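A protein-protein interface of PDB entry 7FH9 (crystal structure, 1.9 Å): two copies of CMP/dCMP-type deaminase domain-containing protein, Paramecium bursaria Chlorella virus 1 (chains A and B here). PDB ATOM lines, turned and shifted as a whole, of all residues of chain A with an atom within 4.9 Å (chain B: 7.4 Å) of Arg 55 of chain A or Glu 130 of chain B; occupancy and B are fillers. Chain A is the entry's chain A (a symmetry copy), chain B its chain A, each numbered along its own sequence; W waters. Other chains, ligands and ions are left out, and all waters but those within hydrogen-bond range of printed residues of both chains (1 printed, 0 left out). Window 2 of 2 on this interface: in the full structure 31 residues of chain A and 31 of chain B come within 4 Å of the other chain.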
ATOM      1  N   LEU A  45     -28.002 -14.309  27.252  1.00  0.00           N
ATOM      2  CA  LEU A  45     -27.260 -15.549  27.401  1.00  0.00           C
ATOM      3  C   LEU A  45     -27.082 -15.845  28.883  1.00  0.00           C
ATOM      4  O   LEU A  45     -27.280 -14.962  29.722  1.00  0.00           O
ATOM      5  CB  LEU A  45     -25.905 -15.440  26.688  1.00  0.00           C
ATOM      6  CG  LEU A  45     -25.918 -14.982  25.219  1.00  0.00           C
ATOM      7  CD1 LEU A  45     -24.556 -15.254  24.547  1.00  0.00           C
ATOM      8  CD2 LEU A  45     -27.066 -15.612  24.406  1.00  0.00           C
ATOM      9  N   PHE A  49     -21.597 -16.359  30.757  1.00  0.00           N
ATOM     10  CA  PHE A  49     -21.226 -16.949  29.477  1.00  0.00           C
ATOM     11  C   PHE A  49     -20.669 -15.856  28.576  1.00  0.00           C
ATOM     12  O   PHE A  49     -21.283 -14.793  28.449  1.00  0.00           O
ATOM     13  CB  PHE A  49     -22.459 -17.597  28.828  1.00  0.00           C
ATOM     14  CG  PHE A  49     -22.138 -18.613  27.761  1.00  0.00           C
ATOM     15  CD1 PHE A  49     -21.381 -19.735  28.063  1.00  0.00           C
ATOM     16  CD2 PHE A  49     -22.639 -18.467  26.472  1.00  0.00           C
ATOM     17  CE1 PHE A  49     -21.111 -20.693  27.096  1.00  0.00           C
ATOM     18  CE2 PHE A  49     -22.379 -19.411  25.500  1.00  0.00           C
ATOM     19  CZ  PHE A  49     -21.606 -20.528  25.810  1.00  0.00           C
ATOM     20  N   GLU A  50     -19.515 -16.111  27.952  1.00  0.00           N
ATOM     21  CA  GLU A  50     -18.868 -15.073  27.147  1.00  0.00           C
ATOM     22  C   GLU A  50     -19.770 -14.692  25.980  1.00  0.00           C
ATOM     23  O   GLU A  50     -20.141 -15.543  25.165  1.00  0.00           O
ATOM     24  CB  GLU A  50     -17.502 -15.538  26.635  1.00  0.00           C
ATOM     25  CG  GLU A  50     -16.762 -14.435  25.862  1.00  0.00           C
ATOM     26  CD  GLU A  50     -15.452 -14.885  25.229  1.00  0.00           C
ATOM     27  OE1 GLU A  50     -15.218 -16.103  25.074  1.00  0.00           O
ATOM     28  OE2 GLU A  50     -14.669 -13.990  24.859  1.00  0.00           O
ATOM     29  N   THR A  52     -19.871 -13.367  22.915  1.00  0.00           N
ATOM     30  CA  THR A  52     -19.161 -12.996  21.701  1.00  0.00           C
ATOM     31  C   THR A  52     -20.143 -12.581  20.611  1.00  0.00           C
ATOM     32  O   THR A  52     -21.327 -12.942  20.629  1.00  0.00           O
ATOM     33  CB  THR A  52     -18.318 -14.160  21.184  1.00  0.00           C
ATOM     34  OG1 THR A  52     -19.199 -15.213  20.757  1.00  0.00           O
ATOM     35  CG2 THR A  52     -17.385 -14.673  22.287  1.00  0.00           C
ATOM     36  N   SER A  53     -19.628 -11.821  19.639  1.00  0.00           N
ATOM     37  CA  SER A  53     -20.444 -11.464  18.482  1.00  0.00           C
ATOM     38  C   SER A  53     -20.995 -12.709  17.796  1.00  0.00           C
ATOM     39  O   SER A  53     -22.180 -12.760  17.440  1.00  0.00           O
ATOM     40  CB  SER A  53     -19.625 -10.623  17.502  1.00  0.00           C
ATOM     41  OG  SER A  53     -20.429 -10.207  16.417  1.00  0.00           O
ATOM     42  N   ASP A  54     -20.157 -13.739  17.640  1.00  0.00           N
ATOM     43  CA  ASP A  54     -20.593 -14.982  17.000  1.00  0.00           C
ATOM     44  C   ASP A  54     -21.740 -15.652  17.751  1.00  0.00           C
ATOM     45  O   ASP A  54     -22.656 -16.204  17.127  1.00  0.00           O
ATOM     46  CB  ASP A  54     -19.409 -15.947  16.861  1.00  0.00           C
ATOM     47  CG  ASP A  54     -18.435 -15.522  15.782  1.00  0.00           C
ATOM     48  OD1 ASP A  54     -18.790 -14.609  15.011  1.00  0.00           O
ATOM     49  OD2 ASP A  54     -17.342 -16.120  15.702  1.00  0.00           O
ATOM     50  N   ARG A  55     -21.714 -15.623  19.088  1.00  0.00           N
ATOM     51  CA  ARG A  55     -22.762 -16.283  19.854  1.00  0.00           C
ATOM     52  C   ARG A  55     -24.089 -15.547  19.783  1.00  0.00           C
ATOM     53  O   ARG A  55     -25.127 -16.164  20.022  1.00  0.00           O
ATOM     54  CB  ARG A  55     -22.342 -16.450  21.321  1.00  0.00           C
ATOM     55  CG  ARG A  55     -21.337 -17.605  21.506  1.00  0.00           C
ATOM     56  CD  ARG A  55     -20.692 -17.637  22.880  1.00  0.00           C
ATOM     57  NE  ARG A  55     -19.923 -18.859  23.081  1.00  0.00           N
ATOM     58  CZ  ARG A  55     -19.215 -19.143  24.166  1.00  0.00           C
ATOM     59  NH1 ARG A  55     -19.166 -18.277  25.166  1.00  0.00           N
ATOM     60  NH2 ARG A  55     -18.570 -20.303  24.249  1.00  0.00           N
ATOM     61  N   TRP A  56     -24.090 -14.262  19.431  1.00  0.00           N
ATOM     62  CA  TRP A  56     -25.325 -13.493  19.336  1.00  0.00           C
ATOM     63  C   TRP A  56     -25.879 -13.412  17.914  1.00  0.00           C
ATOM     64  O   TRP A  56     -26.964 -12.851  17.720  1.00  0.00           O
ATOM     65  CB  TRP A  56     -25.115 -12.076  19.903  1.00  0.00           C
ATOM     66  CG  TRP A  56     -25.461 -11.938  21.376  1.00  0.00           C
ATOM     67  CD1 TRP A  56     -24.606 -11.643  22.402  1.00  0.00           C
ATOM     68  CD2 TRP A  56     -26.757 -12.087  21.969  1.00  0.00           C
ATOM     69  NE1 TRP A  56     -25.291 -11.593  23.592  1.00  0.00           N
ATOM     70  CE2 TRP A  56     -26.610 -11.876  23.355  1.00  0.00           C
ATOM     71  CE3 TRP A  56     -28.026 -12.390  21.459  1.00  0.00           C
ATOM     72  CZ2 TRP A  56     -27.681 -11.941  24.238  1.00  0.00           C
ATOM     73  CZ3 TRP A  56     -29.094 -12.469  22.339  1.00  0.00           C
ATOM     74  CH2 TRP A  56     -28.915 -12.243  23.714  1.00  0.00           C
ATOM     75  N   GLU A  57     -25.171 -13.952  16.923  1.00  0.00           N
ATOM     76  CA  GLU A  57     -25.675 -14.026  15.560  1.00  0.00           C
ATOM     77  C   GLU A  57     -26.725 -15.130  15.441  1.00  0.00           C
ATOM     78  O   GLU A  57     -26.800 -16.044  16.265  1.00  0.00           O
ATOM     79  CB  GLU A  57     -24.541 -14.295  14.568  1.00  0.00           C
ATOM     80  CG  GLU A  57     -23.561 -13.150  14.397  1.00  0.00           C
ATOM     81  CD  GLU A  57     -22.515 -13.420  13.319  1.00  0.00           C
ATOM     82  OE1 GLU A  57     -22.314 -14.598  12.945  1.00  0.00           O
ATOM     83  OE2 GLU A  57     -21.893 -12.447  12.847  1.00  0.00           O
ATOM     84  N   MET A  60     -26.984 -19.092  15.578  1.00  0.00           N
ATOM     85  CA  MET A  60     -26.204 -19.653  16.679  1.00  0.00           C
ATOM     86  C   MET A  60     -26.786 -19.244  18.030  1.00  0.00           C
ATOM     87  O   MET A  60     -26.794 -20.044  18.981  1.00  0.00           O
ATOM     88  CB  MET A  60     -24.730 -19.233  16.543  1.00  0.00           C
ATOM     89  CG  MET A  60     -23.889 -19.567  17.766  1.00  0.00           C
ATOM     90  SD  MET A  60     -23.641 -21.363  17.954  1.00  0.00           S
ATOM     91  CE  MET A  60     -23.395 -21.896  16.260  1.00  0.00           C
ATOM     92  N   LYS A  61     -27.348 -18.034  18.121  1.00  0.00           N
ATOM     93  CA  LYS A  61     -27.802 -17.542  19.422  1.00  0.00           C
ATOM     94  C   LYS A  61     -28.898 -18.411  20.032  1.00  0.00           C
ATOM     95  O   LYS A  61     -29.045 -18.441  21.256  1.00  0.00           O
ATOM     96  CB  LYS A  61     -28.290 -16.092  19.327  1.00  0.00           C
ATOM     97  CG  LYS A  61     -29.599 -15.900  18.575  1.00  0.00           C
ATOM     98  CD  LYS A  61     -29.990 -14.420  18.552  1.00  0.00           C
ATOM     99  CE  LYS A  61     -31.266 -14.178  17.753  1.00  0.00           C
ATOM    100  NZ  LYS A  61     -31.456 -12.716  17.481  1.00  0.00           N
ATOM    101  N   TYR A  64     -28.075 -20.751  22.909  1.00  0.00           N
ATOM    102  CA  TYR A  64     -27.628 -20.201  24.177  1.00  0.00           C
ATOM    103  C   TYR A  64     -28.614 -19.246  24.830  1.00  0.00           C
ATOM    104  O   TYR A  64     -28.506 -19.018  26.039  1.00  0.00           O
ATOM    105  CB  TYR A  64     -26.293 -19.459  23.990  1.00  0.00           C
ATOM    106  CG  TYR A  64     -25.187 -20.287  23.373  1.00  0.00           C
ATOM    107  CD1 TYR A  64     -24.706 -21.433  24.003  1.00  0.00           C
ATOM    108  CD2 TYR A  64     -24.607 -19.913  22.168  1.00  0.00           C
ATOM    109  CE1 TYR A  64     -23.682 -22.185  23.446  1.00  0.00           C
ATOM    110  CE2 TYR A  64     -23.575 -20.658  21.603  1.00  0.00           C
ATOM    111  CZ  TYR A  64     -23.117 -21.791  22.244  1.00  0.00           C
ATOM    112  OH  TYR A  64     -22.089 -22.515  21.673  1.00  0.00           O
ATOM    113  N   ILE B 103     -28.373 -22.847  35.126  1.00  0.00           N
ATOM    114  CA  ILE B 103     -27.391 -21.778  35.332  1.00  0.00           C
ATOM    115  C   ILE B 103     -28.076 -20.531  35.866  1.00  0.00           C
ATOM    116  O   ILE B 103     -27.584 -19.878  36.801  1.00  0.00           O
ATOM    117  CB  ILE B 103     -26.634 -21.473  34.023  1.00  0.00           C
ATOM    118  CG1 ILE B 103     -25.796 -22.674  33.590  1.00  0.00           C
ATOM    119  CG2 ILE B 103     -25.701 -20.254  34.204  1.00  0.00           C
ATOM    120  CD1 ILE B 103     -25.181 -22.523  32.199  1.00  0.00           C
ATOM    121  N   SER B 124     -26.780 -31.576  21.618  1.00  0.00           N
ATOM    122  CA  SER B 124     -27.380 -30.987  22.810  1.00  0.00           C
ATOM    123  C   SER B 124     -26.481 -31.158  24.030  1.00  0.00           C
ATOM    124  O   SER B 124     -26.237 -30.202  24.778  1.00  0.00           O
ATOM    125  CB  SER B 124     -28.743 -31.625  23.058  1.00  0.00           C
ATOM    126  OG  SER B 124     -29.234 -31.295  24.343  1.00  0.00           O
ATOM    127  N   PHE B 125     -26.002 -32.389  24.250  1.00  0.00           N
ATOM    128  CA  PHE B 125     -25.083 -32.686  25.348  1.00  0.00           C
ATOM    129  C   PHE B 125     -23.842 -31.799  25.286  1.00  0.00           C
ATOM    130  O   PHE B 125     -23.358 -31.316  26.316  1.00  0.00           O
ATOM    131  CB  PHE B 125     -24.706 -34.175  25.284  1.00  0.00           C
ATOM    132  CG  PHE B 125     -23.825 -34.663  26.416  1.00  0.00           C
ATOM    133  CD1 PHE B 125     -24.339 -34.837  27.695  1.00  0.00           C
ATOM    134  CD2 PHE B 125     -22.493 -34.993  26.182  1.00  0.00           C
ATOM    135  CE1 PHE B 125     -23.529 -35.303  28.730  1.00  0.00           C
ATOM    136  CE2 PHE B 125     -21.680 -35.459  27.210  1.00  0.00           C
ATOM    137  CZ  PHE B 125     -22.201 -35.614  28.484  1.00  0.00           C
ATOM    138  N   SER B 126     -23.322 -31.561  24.084  1.00  0.00           N
ATOM    139  CA  SER B 126     -22.126 -30.732  23.947  1.00  0.00           C
ATOM    140  C   SER B 126     -22.408 -29.275  24.313  1.00  0.00           C
ATOM    141  O   SER B 126     -21.570 -28.609  24.935  1.00  0.00           O
ATOM    142  CB  SER B 126     -21.592 -30.833  22.520  1.00  0.00           C
ATOM    143  OG  SER B 126     -21.243 -32.174  22.199  1.00  0.00           O
ATOM    144  N   PHE B 127     -23.568 -28.751  23.911  1.00  0.00           N
ATOM    145  CA  PHE B 127     -23.928 -27.379  24.270  1.00  0.00           C
ATOM    146  C   PHE B 127     -24.115 -27.230  25.781  1.00  0.00           C
ATOM    147  O   PHE B 127     -23.630 -26.264  26.382  1.00  0.00           O
ATOM    148  CB  PHE B 127     -25.203 -26.962  23.529  1.00  0.00           C
ATOM    149  CG  PHE B 127     -24.973 -26.526  22.102  1.00  0.00           C
ATOM    150  CD1 PHE B 127     -24.029 -25.555  21.792  1.00  0.00           C
ATOM    151  CD2 PHE B 127     -25.722 -27.081  21.069  1.00  0.00           C
ATOM    152  CE1 PHE B 127     -23.821 -25.153  20.481  1.00  0.00           C
ATOM    153  CE2 PHE B 127     -25.517 -26.686  19.757  1.00  0.00           C
ATOM    154  CZ  PHE B 127     -24.564 -25.721  19.459  1.00  0.00           C
ATOM    155  N   SER B 128     -24.832 -28.169  26.410  1.00  0.00           N
ATOM    156  CA  SER B 128     -25.012 -28.113  27.860  1.00  0.00           C
ATOM    157  C   SER B 128     -23.668 -28.080  28.580  1.00  0.00           C
ATOM    158  O   SER B 128     -23.463 -27.280  29.499  1.00  0.00           O
ATOM    159  CB  SER B 128     -25.840 -29.305  28.350  1.00  0.00           C
ATOM    160  OG  SER B 128     -27.147 -29.283  27.806  1.00  0.00           O
ATOM    161  N   ASN B 129     -22.738 -28.947  28.178  1.00  0.00           N
ATOM    162  CA  ASN B 129     -21.463 -29.013  28.882  1.00  0.00           C
ATOM    163  C   ASN B 129     -20.581 -27.811  28.572  1.00  0.00           C
ATOM    164  O   ASN B 129     -19.803 -27.377  29.431  1.00  0.00           O
ATOM    165  CB  ASN B 129     -20.756 -30.325  28.554  1.00  0.00           C
ATOM    166  CG  ASN B 129     -21.326 -31.490  29.357  1.00  0.00           C
ATOM    167  OD1 ASN B 129     -21.066 -31.612  30.555  1.00  0.00           O
ATOM    168  ND2 ASN B 129     -22.125 -32.332  28.707  1.00  0.00           N
ATOM    169  N   GLU B 130     -20.706 -27.243  27.370  1.00  0.00           N
ATOM    170  CA  GLU B 130     -19.986 -26.010  27.066  1.00  0.00           C
ATOM    171  C   GLU B 130     -20.433 -24.883  27.992  1.00  0.00           C
ATOM    172  O   GLU B 130     -19.602 -24.132  28.523  1.00  0.00           O
ATOM    173  CB  GLU B 130     -20.195 -25.616  25.600  1.00  0.00           C
ATOM    174  CG  GLU B 130     -19.524 -24.289  25.223  1.00  0.00           C
ATOM    175  CD  GLU B 130     -19.865 -23.849  23.811  1.00  0.00           C
ATOM    176  OE1 GLU B 130     -18.997 -23.278  23.136  1.00  0.00           O
ATOM    177  OE2 GLU B 130     -21.006 -24.092  23.378  1.00  0.00           O
ATOM    178  N   MET B 131     -21.745 -24.737  28.178  1.00  0.00           N
ATOM    179  CA  MET B 131     -22.262 -23.692  29.063  1.00  0.00           C
ATOM    180  C   MET B 131     -21.893 -23.969  30.518  1.00  0.00           C
ATOM    181  O   MET B 131     -21.500 -23.049  31.245  1.00  0.00           O
ATOM    182  CB  MET B 131     -23.781 -23.569  28.908  1.00  0.00           C
ATOM    183  CG  MET B 131     -24.229 -23.100  27.512  1.00  0.00           C
ATOM    184  SD  MET B 131     -25.995 -22.716  27.390  1.00  0.00           S
ATOM    185  CE  MET B 131     -26.663 -24.330  26.975  1.00  0.00           C
ATOM    186  N   PHE B 132     -22.038 -25.227  30.963  1.00  0.00           N
ATOM    187  CA  PHE B 132     -21.696 -25.592  32.339  1.00  0.00           C
ATOM    188  C   PHE B 132     -20.222 -25.317  32.630  1.00  0.00           C
ATOM    189  O   PHE B 132     -19.879 -24.743  33.672  1.00  0.00           O
ATOM    190  CB  PHE B 132     -22.010 -27.077  32.603  1.00  0.00           C
ATOM    191  CG  PHE B 132     -23.493 -27.403  32.750  1.00  0.00           C
ATOM    192  CD1 PHE B 132     -24.427 -26.418  33.056  1.00  0.00           C
ATOM    193  CD2 PHE B 132     -23.940 -28.712  32.594  1.00  0.00           C
ATOM    194  CE1 PHE B 132     -25.774 -26.729  33.199  1.00  0.00           C
ATOM    195  CE2 PHE B 132     -25.289 -29.035  32.734  1.00  0.00           C
ATOM    196  CZ  PHE B 132     -26.206 -28.044  33.043  1.00  0.00           C
ATOM    197  N   ASP B 133     -19.331 -25.742  31.727  1.00  0.00           N
ATOM    198  CA  ASP B 133     -17.899 -25.536  31.934  1.00  0.00           C
ATOM    199  C   ASP B 133     -17.567 -24.055  32.054  1.00  0.00           C
ATOM    200  O   ASP B 133     -16.806 -23.647  32.937  1.00  0.00           O
ATOM    201  CB  ASP B 133     -17.104 -26.154  30.783  1.00  0.00           C
ATOM    202  CG  ASP B 133     -16.983 -27.658  30.896  1.00  0.00           C
ATOM    203  OD1 ASP B 133     -17.246 -28.194  31.991  1.00  0.00           O
ATOM    204  OD2 ASP B 133     -16.614 -28.307  29.892  1.00  0.00           O
ATOM    205  N   GLU B 134     -18.144 -23.233  31.178  1.00  0.00           N
ATOM    206  CA  GLU B 134     -17.803 -21.821  31.143  1.00  0.00           C
ATOM    207  C   GLU B 134     -18.425 -21.066  32.315  1.00  0.00           C
ATOM    208  O   GLU B 134     -17.811 -20.136  32.854  1.00  0.00           O
ATOM    209  CB  GLU B 134     -18.255 -21.231  29.810  1.00  0.00           C
ATOM    210  CG  GLU B 134     -17.600 -19.953  29.464  1.00  0.00           C
ATOM    211  CD  GLU B 134     -17.785 -19.571  28.006  1.00  0.00           C
ATOM    212  OE1 GLU B 134     -17.656 -20.441  27.113  1.00  0.00           O
ATOM    213  OE2 GLU B 134     -18.060 -18.383  27.760  1.00  0.00           O
ATOM    214  N   CYS B 135     -19.627 -21.461  32.736  1.00  0.00           N
ATOM    215  CA  CYS B 135     -20.376 -20.730  33.753  1.00  0.00           C
ATOM    216  C   CYS B 135     -20.131 -21.243  35.168  1.00  0.00           C
ATOM    217  O   CYS B 135     -20.740 -20.724  36.111  1.00  0.00           O
ATOM    218  CB  CYS B 135     -21.880 -20.783  33.429  1.00  0.00           C
ATOM    219  SG  CYS B 135     -22.259 -19.944  31.857  1.00  0.00           S
ATOM    220  N   GLY B 136     -19.274 -22.247  35.336  1.00  0.00           N
ATOM    221  CA  GLY B 136     -18.895 -22.707  36.657  1.00  0.00           C
ATOM    222  C   GLY B 136     -19.786 -23.759  37.279  1.00  0.00           C
ATOM    223  O   GLY B 136     -19.854 -23.846  38.509  1.00  0.00           O
HETATM  224  O   HOH W   1     -15.542 -18.473  25.789  1.00  0.00           O
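No position is printed for both chains. Of the 9 pairs that touch across the chains among the printed residues, none has its exchanged pair printed and touching as well.
The backbone NH (N) of Arg 55 of chain A lies within hydrogen-bond range of the side-chain hydroxyl (OG1) of Thr 52 of chain A (3.0 Å). The backbone carbonyl oxygen (O) of Arg 55 of chain A lies close to the backbone NH (N) of Lys 61 of chain A (3.5 Å). NH1 of Arg 55 of chain A sits at hydrogen-bond distance from O of Glu 50 of chain A, at 2.9 Å. The side-chain sulfur (SG) of Cys 135 of chain B sits close to the backbone carbonyl oxygen (O) of Met 131 of chain B.
Water W1 lies within hydrogen-bond range of the side-chain carboxylate of Glu 50 of chain A (2.5 Å) and the side-chain carboxylate of Glu 134 of chain B (3.2 Å).
Of the 14 printed residues of chain B, 5 touch a printed residue of chain A. Printed residues of chain A that touch a printed residue of chain B: Phe 49, Glu 50, Arg 55 and Tyr 64. Hydrophobic or aromatic side chains of chain A within 4 Å of the printed part of chain B: Phe 49 and Tyr 64.
CA of Met 131 of chain B touches CE1 of Phe 49 of chain A (3.8 Å). OE1 of Glu 134 of chain B touches CE1 of Phe 49 of chain A, 3.5 Å away. Cys 135 of chain B touches Phe 49 of chain A (SG to N, 3.8 Å). OH of Tyr 64 of chain A touches CE1 of Phe 127 of chain B, 3.4 Å away. CD1 of Tyr 64 of chain A touches SD of Met 131 of chain B, 3.8 Å away.
Leu 45 of chain A touches none of the printed residues of chain B. Printed residues of chain B within 4 Å of Phe 49 of chain A: Met 131 (3.8 Å), Glu 134 (3.5 Å) and Cys 135 (3.8 Å). Of the printed residues of chain B, Glu 50 of chain A touches Glu 134 (2.7 Å). Arg 55 of chain A touches just these residues of chain B: Glu 130 and Glu 134. Printed residues of chain A within 4 Å of Phe 127 of chain B: Tyr 64 (3.4 Å). Of the printed residues of chain A, Glu 130 of chain B touches Arg 55 and Tyr 64. Of the printed residues of chain A, Met 131 of chain B touches Phe 49 and Tyr 64. The nearest residue of chain B that does not touch Arg 55 of chain A is Met 131 of chain B (6.7 Å).
The guanidinium group (NH1) of Arg 55 of chain A is in salt-bridge range of the side-chain carboxylate (OE2) of Glu 134 of chain B (2.8 Å). The side-chain carboxylate of Glu 130 of chain B lies within hydrogen-bond range of the side-chain hydroxyl of Tyr 64 of chain A. The side-chain carboxylate (OE1) of Glu 130 of chain B is in salt-bridge range of the guanidinium group (NH2) of Arg 55 of chain A, 3.2 Å away. OE2 of Glu 134 of chain B sits at hydrogen-bond distance from N of Glu 50 of chain A, 2.7 Å away.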
